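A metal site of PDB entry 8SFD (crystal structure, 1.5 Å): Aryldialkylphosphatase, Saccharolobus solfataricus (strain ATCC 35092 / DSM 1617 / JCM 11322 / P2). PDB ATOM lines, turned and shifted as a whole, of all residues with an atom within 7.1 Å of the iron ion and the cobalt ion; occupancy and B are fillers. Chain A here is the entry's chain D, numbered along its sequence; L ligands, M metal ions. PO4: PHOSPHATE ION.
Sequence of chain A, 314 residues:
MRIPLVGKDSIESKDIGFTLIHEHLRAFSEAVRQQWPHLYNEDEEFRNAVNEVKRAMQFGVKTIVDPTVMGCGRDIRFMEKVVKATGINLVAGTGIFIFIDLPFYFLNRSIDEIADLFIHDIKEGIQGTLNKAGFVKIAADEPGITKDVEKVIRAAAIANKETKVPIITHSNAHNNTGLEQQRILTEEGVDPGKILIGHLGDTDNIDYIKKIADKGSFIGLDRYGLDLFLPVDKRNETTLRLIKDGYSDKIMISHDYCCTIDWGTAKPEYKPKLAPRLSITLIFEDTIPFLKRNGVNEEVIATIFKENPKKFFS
NZ of KCX 137 sits at hydrogen-bond distance from O of Pro 67 (3.4 Å). N of His 24 is in hydrogen-bond range of O of Tyr 257 (3.0 Å). The side-chain carboxylate of Asp 222 is in hydrogen-bond range of a ring nitrogen (ND1) of His 199. A ring nitrogen (NE2) of His 170 lies within hydrogen-bond range of the side-chain carboxylate (OD2) of Asp 141. N of His 170 sits at hydrogen-bond distance from O of Ile 138. The side-chain carboxylate (OD2) of Asp 256 lies within salt-bridge range of the guanidinium group (NE) of Arg 223 (2.9 Å). OE2 of Glu 23 lies within hydrogen-bond range of N of Asp 256, at 3.3 Å. N of Asp 256 is in hydrogen-bond range of O of Asp 222 (3.1 Å).
The nearest printed residue that does not touch the iron ion is His 199 (4.4 Å).
Arg 223 touches the cobalt ion. Of the 22 residues printed, 4 come within 4 Å of the cobalt ion. Along chain A the residues within 4 Å of the cobalt ion span positions 137 to 223. The nearest printed residue that does not touch the cobalt ion is Phe 97 (4.001 Å).
The iron ion is bound by O2 of the ligand (2.0 Å), NE2 of His 24 (2.0 Å), OQ1 of KCX 137 (2.1 Å), NE2 of His 22 (2.1 Å), OD1 of Asp 256 (2.2 Å) and O3 of the ligand (2.4 Å).
The cobalt ion is bound by an oxygen (O2) of the ligand (1.9 Å), OQ2 of KCX 137 (2.0 Å), a ring nitrogen (NE2) of His 199 (2.1 Å), a ring nitrogen (ND1) of His 170 (2.1 Å) and an oxygen (O4) of the ligand (2.5 Å).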
ATOM      1  N   HIS A  22       5.332  16.377 -21.387  1.00  0.00           N
ATOM      2  CA  HIS A  22       5.882  17.062 -20.221  1.00  0.00           C
ATOM      3  C   HIS A  22       4.774  17.771 -19.440  1.00  0.00           C
ATOM      4  O   HIS A  22       4.455  18.932 -19.711  1.00  0.00           O
ATOM      5  CB  HIS A  22       6.987  18.051 -20.629  1.00  0.00           C
ATOM      6  CG  HIS A  22       7.793  18.617 -19.502  1.00  0.00           C
ATOM      7  ND1 HIS A  22       9.160  18.769 -19.578  1.00  0.00           N
ATOM      8  CD2 HIS A  22       7.446  19.080 -18.280  1.00  0.00           C
ATOM      9  CE1 HIS A  22       9.616  19.297 -18.456  1.00  0.00           C
ATOM     10  NE2 HIS A  22       8.591  19.497 -17.653  1.00  0.00           N
ATOM     11  N   GLU A  23       4.208  17.058 -18.462  1.00  0.00           N
ATOM     12  CA  GLU A  23       3.208  17.603 -17.548  1.00  0.00           C
ATOM     13  C   GLU A  23       3.496  17.101 -16.139  1.00  0.00           C
ATOM     14  O   GLU A  23       4.093  16.039 -15.973  1.00  0.00           O
ATOM     15  CB  GLU A  23       1.802  17.180 -17.980  1.00  0.00           C
ATOM     16  CG  GLU A  23       1.497  17.404 -19.449  1.00  0.00           C
ATOM     17  CD  GLU A  23       1.410  18.866 -19.858  1.00  0.00           C
ATOM     18  OE1 GLU A  23       1.432  19.131 -21.080  1.00  0.00           O
ATOM     19  OE2 GLU A  23       1.298  19.725 -18.961  1.00  0.00           O
ATOM     20  N   HIS A  24       3.052  17.860 -15.127  1.00  0.00           N
ATOM     21  CA  HIS A  24       3.243  17.464 -13.737  1.00  0.00           C
ATOM     22  C   HIS A  24       1.897  17.337 -13.042  1.00  0.00           C
ATOM     23  O   HIS A  24       1.160  18.313 -12.925  1.00  0.00           O
ATOM     24  CB  HIS A  24       4.083  18.500 -12.989  1.00  0.00           C
ATOM     25  CG  HIS A  24       5.453  18.712 -13.542  1.00  0.00           C
ATOM     26  ND1 HIS A  24       6.555  17.976 -13.146  1.00  0.00           N
ATOM     27  CD2 HIS A  24       5.913  19.597 -14.435  1.00  0.00           C
ATOM     28  CE1 HIS A  24       7.620  18.401 -13.808  1.00  0.00           C
ATOM     29  NE2 HIS A  24       7.262  19.379 -14.598  1.00  0.00           N
ATOM     30  N   PRO A  67       7.582  14.272 -15.833  1.00  0.00           N
ATOM     31  CA  PRO A  67       8.991  14.292 -15.449  1.00  0.00           C
ATOM     32  C   PRO A  67       9.284  14.897 -14.075  1.00  0.00           C
ATOM     33  O   PRO A  67      10.275  15.600 -13.895  1.00  0.00           O
ATOM     34  CB  PRO A  67       9.617  15.140 -16.573  1.00  0.00           C
ATOM     35  CG  PRO A  67       8.526  16.106 -16.980  1.00  0.00           C
ATOM     36  CD  PRO A  67       7.214  15.410 -16.690  1.00  0.00           C
ATOM     37  N   THR A  68       8.403  14.599 -13.114  1.00  0.00           N
ATOM     38  CA  THR A  68       8.615  14.946 -11.714  1.00  0.00           C
ATOM     39  C   THR A  68       9.595  13.945 -11.104  1.00  0.00           C
ATOM     40  O   THR A  68       9.288  12.757 -11.058  1.00  0.00           O
ATOM     41  CB  THR A  68       7.297  14.931 -10.930  1.00  0.00           C
ATOM     42  OG1 THR A  68       6.294  15.698 -11.615  1.00  0.00           O
ATOM     43  CG2 THR A  68       7.466  15.467  -9.523  1.00  0.00           C
ATOM     44  N   PHE A  97      16.707  16.665 -10.078  1.00  0.00           N
ATOM     45  CA  PHE A  97      16.446  18.030 -10.516  1.00  0.00           C
ATOM     46  C   PHE A  97      17.181  18.991  -9.596  1.00  0.00           C
ATOM     47  O   PHE A  97      16.713  19.271  -8.487  1.00  0.00           O
ATOM     48  CB  PHE A  97      14.933  18.264 -10.551  1.00  0.00           C
ATOM     49  CG  PHE A  97      14.494  19.529 -11.228  1.00  0.00           C
ATOM     50  CD1 PHE A  97      14.554  20.759 -10.570  1.00  0.00           C
ATOM     51  CD2 PHE A  97      14.028  19.505 -12.525  1.00  0.00           C
ATOM     52  CE1 PHE A  97      14.149  21.918 -11.207  1.00  0.00           C
ATOM     53  CE2 PHE A  97      13.627  20.677 -13.158  1.00  0.00           C
ATOM     54  CZ  PHE A  97      13.692  21.873 -12.495  1.00  0.00           C
ATOM     55  N   PHE A  99      19.931  22.707  -9.743  1.00  0.00           N
ATOM     56  CA  PHE A  99      20.519  23.783 -10.527  1.00  0.00           C
ATOM     57  C   PHE A  99      21.958  24.064 -10.093  1.00  0.00           C
ATOM     58  O   PHE A  99      22.711  24.639 -10.877  1.00  0.00           O
ATOM     59  CB  PHE A  99      19.695  25.060 -10.396  1.00  0.00           C
ATOM     60  CG  PHE A  99      18.343  25.033 -11.047  1.00  0.00           C
ATOM     61  CD1 PHE A  99      17.950  23.977 -11.857  1.00  0.00           C
ATOM     62  CD2 PHE A  99      17.442  26.072 -10.849  1.00  0.00           C
ATOM     63  CE1 PHE A  99      16.696  23.956 -12.451  1.00  0.00           C
ATOM     64  CE2 PHE A  99      16.188  26.051 -11.444  1.00  0.00           C
ATOM     65  CZ  PHE A  99      15.813  25.000 -12.238  1.00  0.00           C
ATOM     66  N   KCX A 137      15.209  12.174 -16.210  1.00  0.00           N
ATOM     67  CA  KCX A 137      15.045  13.649 -16.209  1.00  0.00           C
ATOM     68  CB  KCX A 137      13.764  14.044 -15.482  1.00  0.00           C
ATOM     69  CG  KCX A 137      13.595  15.548 -15.242  1.00  0.00           C
ATOM     70  CD  KCX A 137      13.397  16.337 -16.519  1.00  0.00           C
ATOM     71  CE  KCX A 137      13.167  17.814 -16.276  1.00  0.00           C
ATOM     72  NZ  KCX A 137      11.898  18.094 -15.621  1.00  0.00           N
ATOM     73  C   KCX A 137      16.267  14.294 -15.555  1.00  0.00           C
ATOM     74  O   KCX A 137      16.641  13.862 -14.447  1.00  0.00           O
ATOM     75  CX  KCX A 137      11.339  19.315 -15.680  1.00  0.00           C
ATOM     76  OQ1 KCX A 137      10.188  19.374 -15.004  1.00  0.00           O
ATOM     77  OQ2 KCX A 137      11.816  20.252 -16.278  1.00  0.00           O
ATOM     78  N   ILE A 138      16.848  15.306 -16.241  1.00  0.00           N
ATOM     79  CA  ILE A 138      18.001  16.103 -15.724  1.00  0.00           C
ATOM     80  C   ILE A 138      17.701  17.583 -15.944  1.00  0.00           C
ATOM     81  O   ILE A 138      16.820  17.917 -16.734  1.00  0.00           O
ATOM     82  CB  ILE A 138      19.317  15.667 -16.401  1.00  0.00           C
ATOM     83  CG1 ILE A 138      19.306  15.987 -17.896  1.00  0.00           C
ATOM     84  CG2 ILE A 138      19.607  14.193 -16.133  1.00  0.00           C
ATOM     85  CD1 ILE A 138      20.597  15.648 -18.616  1.00  0.00           C
ATOM     86  N   ALA A 139      18.442  18.448 -15.242  1.00  0.00           N
ATOM     87  CA  ALA A 139      18.186  19.883 -15.293  1.00  0.00           C
ATOM     88  C   ALA A 139      19.483  20.685 -15.250  1.00  0.00           C
ATOM     89  O   ALA A 139      20.494  20.237 -14.731  1.00  0.00           O
ATOM     90  CB  ALA A 139      17.281  20.281 -14.154  1.00  0.00           C
ATOM     91  N   ASP A 141      20.079  25.378 -15.278  1.00  0.00           N
ATOM     92  CA  ASP A 141      19.382  26.645 -15.429  1.00  0.00           C
ATOM     93  C   ASP A 141      20.398  27.776 -15.381  1.00  0.00           C
ATOM     94  O   ASP A 141      21.499  27.637 -15.902  1.00  0.00           O
ATOM     95  CB  ASP A 141      18.263  26.764 -14.389  1.00  0.00           C
ATOM     96  CG  ASP A 141      17.133  27.695 -14.791  1.00  0.00           C
ATOM     97  OD1 ASP A 141      17.288  28.923 -14.604  1.00  0.00           O
ATOM     98  OD2 ASP A 141      16.116  27.192 -15.307  1.00  0.00           O
ATOM     99  N   THR A 169      15.212  16.791 -20.654  1.00  0.00           N
ATOM    100  CA  THR A 169      15.931  17.793 -19.888  1.00  0.00           C
ATOM    101  C   THR A 169      15.068  19.020 -19.612  1.00  0.00           C
ATOM    102  O   THR A 169      14.097  19.312 -20.311  1.00  0.00           O
ATOM    103  CB  THR A 169      17.242  18.249 -20.561  1.00  0.00           C
ATOM    104  OG1 THR A 169      16.974  19.345 -21.444  1.00  0.00           O
ATOM    105  CG2 THR A 169      17.942  17.129 -21.291  1.00  0.00           C
ATOM    106  N   HIS A 170      15.445  19.691 -18.522  1.00  0.00           N
ATOM    107  CA  HIS A 170      15.088  21.069 -18.247  1.00  0.00           C
ATOM    108  C   HIS A 170      16.312  21.929 -18.578  1.00  0.00           C
ATOM    109  O   HIS A 170      17.406  21.593 -18.147  1.00  0.00           O
ATOM    110  CB  HIS A 170      14.737  21.206 -16.754  1.00  0.00           C
ATOM    111  CG  HIS A 170      14.634  22.599 -16.249  1.00  0.00           C
ATOM    112  ND1 HIS A 170      13.428  23.132 -15.832  1.00  0.00           N
ATOM    113  CD2 HIS A 170      15.541  23.572 -16.079  1.00  0.00           C
ATOM    114  CE1 HIS A 170      13.612  24.374 -15.422  1.00  0.00           C
ATOM    115  NE2 HIS A 170      14.892  24.663 -15.558  1.00  0.00           N
ATOM    116  N   SER A 171      16.112  22.992 -19.363  1.00  0.00           N
ATOM    117  CA  SER A 171      17.175  23.948 -19.629  1.00  0.00           C
ATOM    118  C   SER A 171      16.655  25.372 -19.469  1.00  0.00           C
ATOM    119  O   SER A 171      15.448  25.591 -19.369  1.00  0.00           O
ATOM    120  CB  SER A 171      17.804  23.725 -21.001  1.00  0.00           C
ATOM    121  OG  SER A 171      17.054  24.345 -22.036  1.00  0.00           O
ATOM    122  N   GLY A 198      14.665  20.528 -23.158  1.00  0.00           N
ATOM    123  CA  GLY A 198      13.445  21.156 -22.680  1.00  0.00           C
ATOM    124  C   GLY A 198      13.506  22.683 -22.605  1.00  0.00           C
ATOM    125  O   GLY A 198      14.573  23.276 -22.451  1.00  0.00           O
ATOM    126  N   HIS A 199      12.315  23.284 -22.739  1.00  0.00           N
ATOM    127  CA  HIS A 199      12.053  24.675 -22.400  1.00  0.00           C
ATOM    128  C   HIS A 199      12.605  25.622 -23.457  1.00  0.00           C
ATOM    129  O   HIS A 199      12.799  26.802 -23.198  1.00  0.00           O
ATOM    130  CB  HIS A 199      12.576  24.996 -20.992  1.00  0.00           C
ATOM    131  CG  HIS A 199      11.990  24.115 -19.936  1.00  0.00           C
ATOM    132  ND1 HIS A 199      10.789  23.458 -20.094  1.00  0.00           N
ATOM    133  CD2 HIS A 199      12.428  23.805 -18.707  1.00  0.00           C
ATOM    134  CE1 HIS A 199      10.536  22.748 -18.994  1.00  0.00           C
ATOM    135  NE2 HIS A 199      11.512  22.952 -18.146  1.00  0.00           N
ATOM    136  N   ASP A 222       7.422  23.579 -24.649  1.00  0.00           N
ATOM    137  CA  ASP A 222       6.817  22.688 -23.676  1.00  0.00           C
ATOM    138  C   ASP A 222       6.287  23.424 -22.448  1.00  0.00           C
ATOM    139  O   ASP A 222       6.004  22.773 -21.441  1.00  0.00           O
ATOM    140  CB  ASP A 222       7.805  21.600 -23.263  1.00  0.00           C
ATOM    141  CG  ASP A 222       9.137  22.127 -22.728  1.00  0.00           C
ATOM    142  OD1 ASP A 222       9.183  23.313 -22.344  1.00  0.00           O
ATOM    143  OD2 ASP A 222      10.103  21.344 -22.703  1.00  0.00           O
ATOM    144  N   ARG A 223       6.090  24.753 -22.520  1.00  0.00           N
ATOM    145  CA  ARG A 223       5.650  25.490 -21.346  1.00  0.00           C
ATOM    146  C   ARG A 223       4.443  26.372 -21.674  1.00  0.00           C
ATOM    147  O   ARG A 223       4.304  27.474 -21.151  1.00  0.00           O
ATOM    148  CB  ARG A 223       6.811  26.308 -20.774  1.00  0.00           C
ATOM    149  CG  ARG A 223       7.712  25.501 -19.850  1.00  0.00           C
ATOM    150  CD  ARG A 223       8.869  26.305 -19.283  1.00  0.00           C
ATOM    151  NE  ARG A 223       9.237  25.846 -17.954  1.00  0.00           N
ATOM    152  CZ  ARG A 223      10.272  26.309 -17.255  1.00  0.00           C
ATOM    153  NH1 ARG A 223      11.082  27.197 -17.787  1.00  0.00           N
ATOM    154  NH2 ARG A 223      10.479  25.868 -16.028  1.00  0.00           N
ATOM    155  N   LEU A 226       2.411  27.598 -18.534  1.00  0.00           N
ATOM    156  CA  LEU A 226       3.016  28.515 -17.577  1.00  0.00           C
ATOM    157  C   LEU A 226       3.024  29.918 -18.165  1.00  0.00           C
ATOM    158  O   LEU A 226       3.206  30.087 -19.368  1.00  0.00           O
ATOM    159  CB  LEU A 226       4.437  28.055 -17.253  1.00  0.00           C
ATOM    160  CG  LEU A 226       4.583  26.648 -16.661  1.00  0.00           C
ATOM    161  CD1 LEU A 226       6.004  26.420 -16.172  1.00  0.00           C
ATOM    162  CD2 LEU A 226       3.586  26.420 -15.539  1.00  0.00           C
ATOM    163  N   ASP A 256       3.811  21.829 -19.449  1.00  0.00           N
ATOM    164  CA  ASP A 256       4.547  21.901 -18.199  1.00  0.00           C
ATOM    165  C   ASP A 256       3.586  22.398 -17.128  1.00  0.00           C
ATOM    166  O   ASP A 256       3.980  23.079 -16.183  1.00  0.00           O
ATOM    167  CB  ASP A 256       5.777  22.803 -18.328  1.00  0.00           C
ATOM    168  CG  ASP A 256       6.853  22.580 -17.276  1.00  0.00           C
ATOM    169  OD1 ASP A 256       6.771  21.599 -16.512  1.00  0.00           O
ATOM    170  OD2 ASP A 256       7.793  23.395 -17.245  1.00  0.00           O
ATOM    171  N   TYR A 257       2.296  22.084 -17.310  1.00  0.00           N
ATOM    172  CA  TYR A 257       1.290  22.504 -16.353  1.00  0.00           C
ATOM    173  C   TYR A 257       1.440  21.663 -15.088  1.00  0.00           C
ATOM    174  O   TYR A 257       1.539  20.441 -15.149  1.00  0.00           O
ATOM    175  CB  TYR A 257      -0.124  22.384 -16.927  1.00  0.00           C
ATOM    176  CG  TYR A 257      -1.187  22.958 -16.021  1.00  0.00           C
ATOM    177  CD1 TYR A 257      -1.249  24.319 -15.780  1.00  0.00           C
ATOM    178  CD2 TYR A 257      -2.084  22.141 -15.359  1.00  0.00           C
ATOM    179  CE1 TYR A 257      -2.194  24.863 -14.930  1.00  0.00           C
ATOM    180  CE2 TYR A 257      -3.039  22.665 -14.509  1.00  0.00           C
ATOM    181  CZ  TYR A 257      -3.104  24.027 -14.298  1.00  0.00           C
ATOM    182  OH  TYR A 257      -4.053  24.558 -13.451  1.00  0.00           O
ATOM    183  N   CYS A 258       1.467  22.357 -13.947  1.00  0.00           N
ATOM    184  CA  CYS A 258       1.445  21.702 -12.647  1.00  0.00           C
ATOM    185  C   CYS A 258       0.037  21.799 -12.083  1.00  0.00           C
ATOM    186  O   CYS A 258      -0.437  22.894 -11.758  1.00  0.00           O
ATOM    187  CB  CYS A 258       2.460  22.351 -11.704  1.00  0.00           C
ATOM    188  SG  CYS A 258       4.144  22.359 -12.366  1.00  0.00           S
HETATM  189  P   PO4 L   1       9.564  22.665 -14.494  1.00  0.00           P
HETATM  190  O1  PO4 L   1       8.832  24.009 -14.574  1.00  0.00           O
HETATM  191  O2  PO4 L   1       9.735  22.071 -15.896  1.00  0.00           O
HETATM  192  O3  PO4 L   1       8.746  21.700 -13.640  1.00  0.00           O
HETATM  193  O4  PO4 L   1      10.939  22.869 -13.871  1.00  0.00           O
HETATM  194 FE    FE M   1       8.535  20.479 -15.752  1.00  0.00          FE
HETATM  195 CO    CO M   2      11.569  22.257 -16.204  1.00  0.00          CO
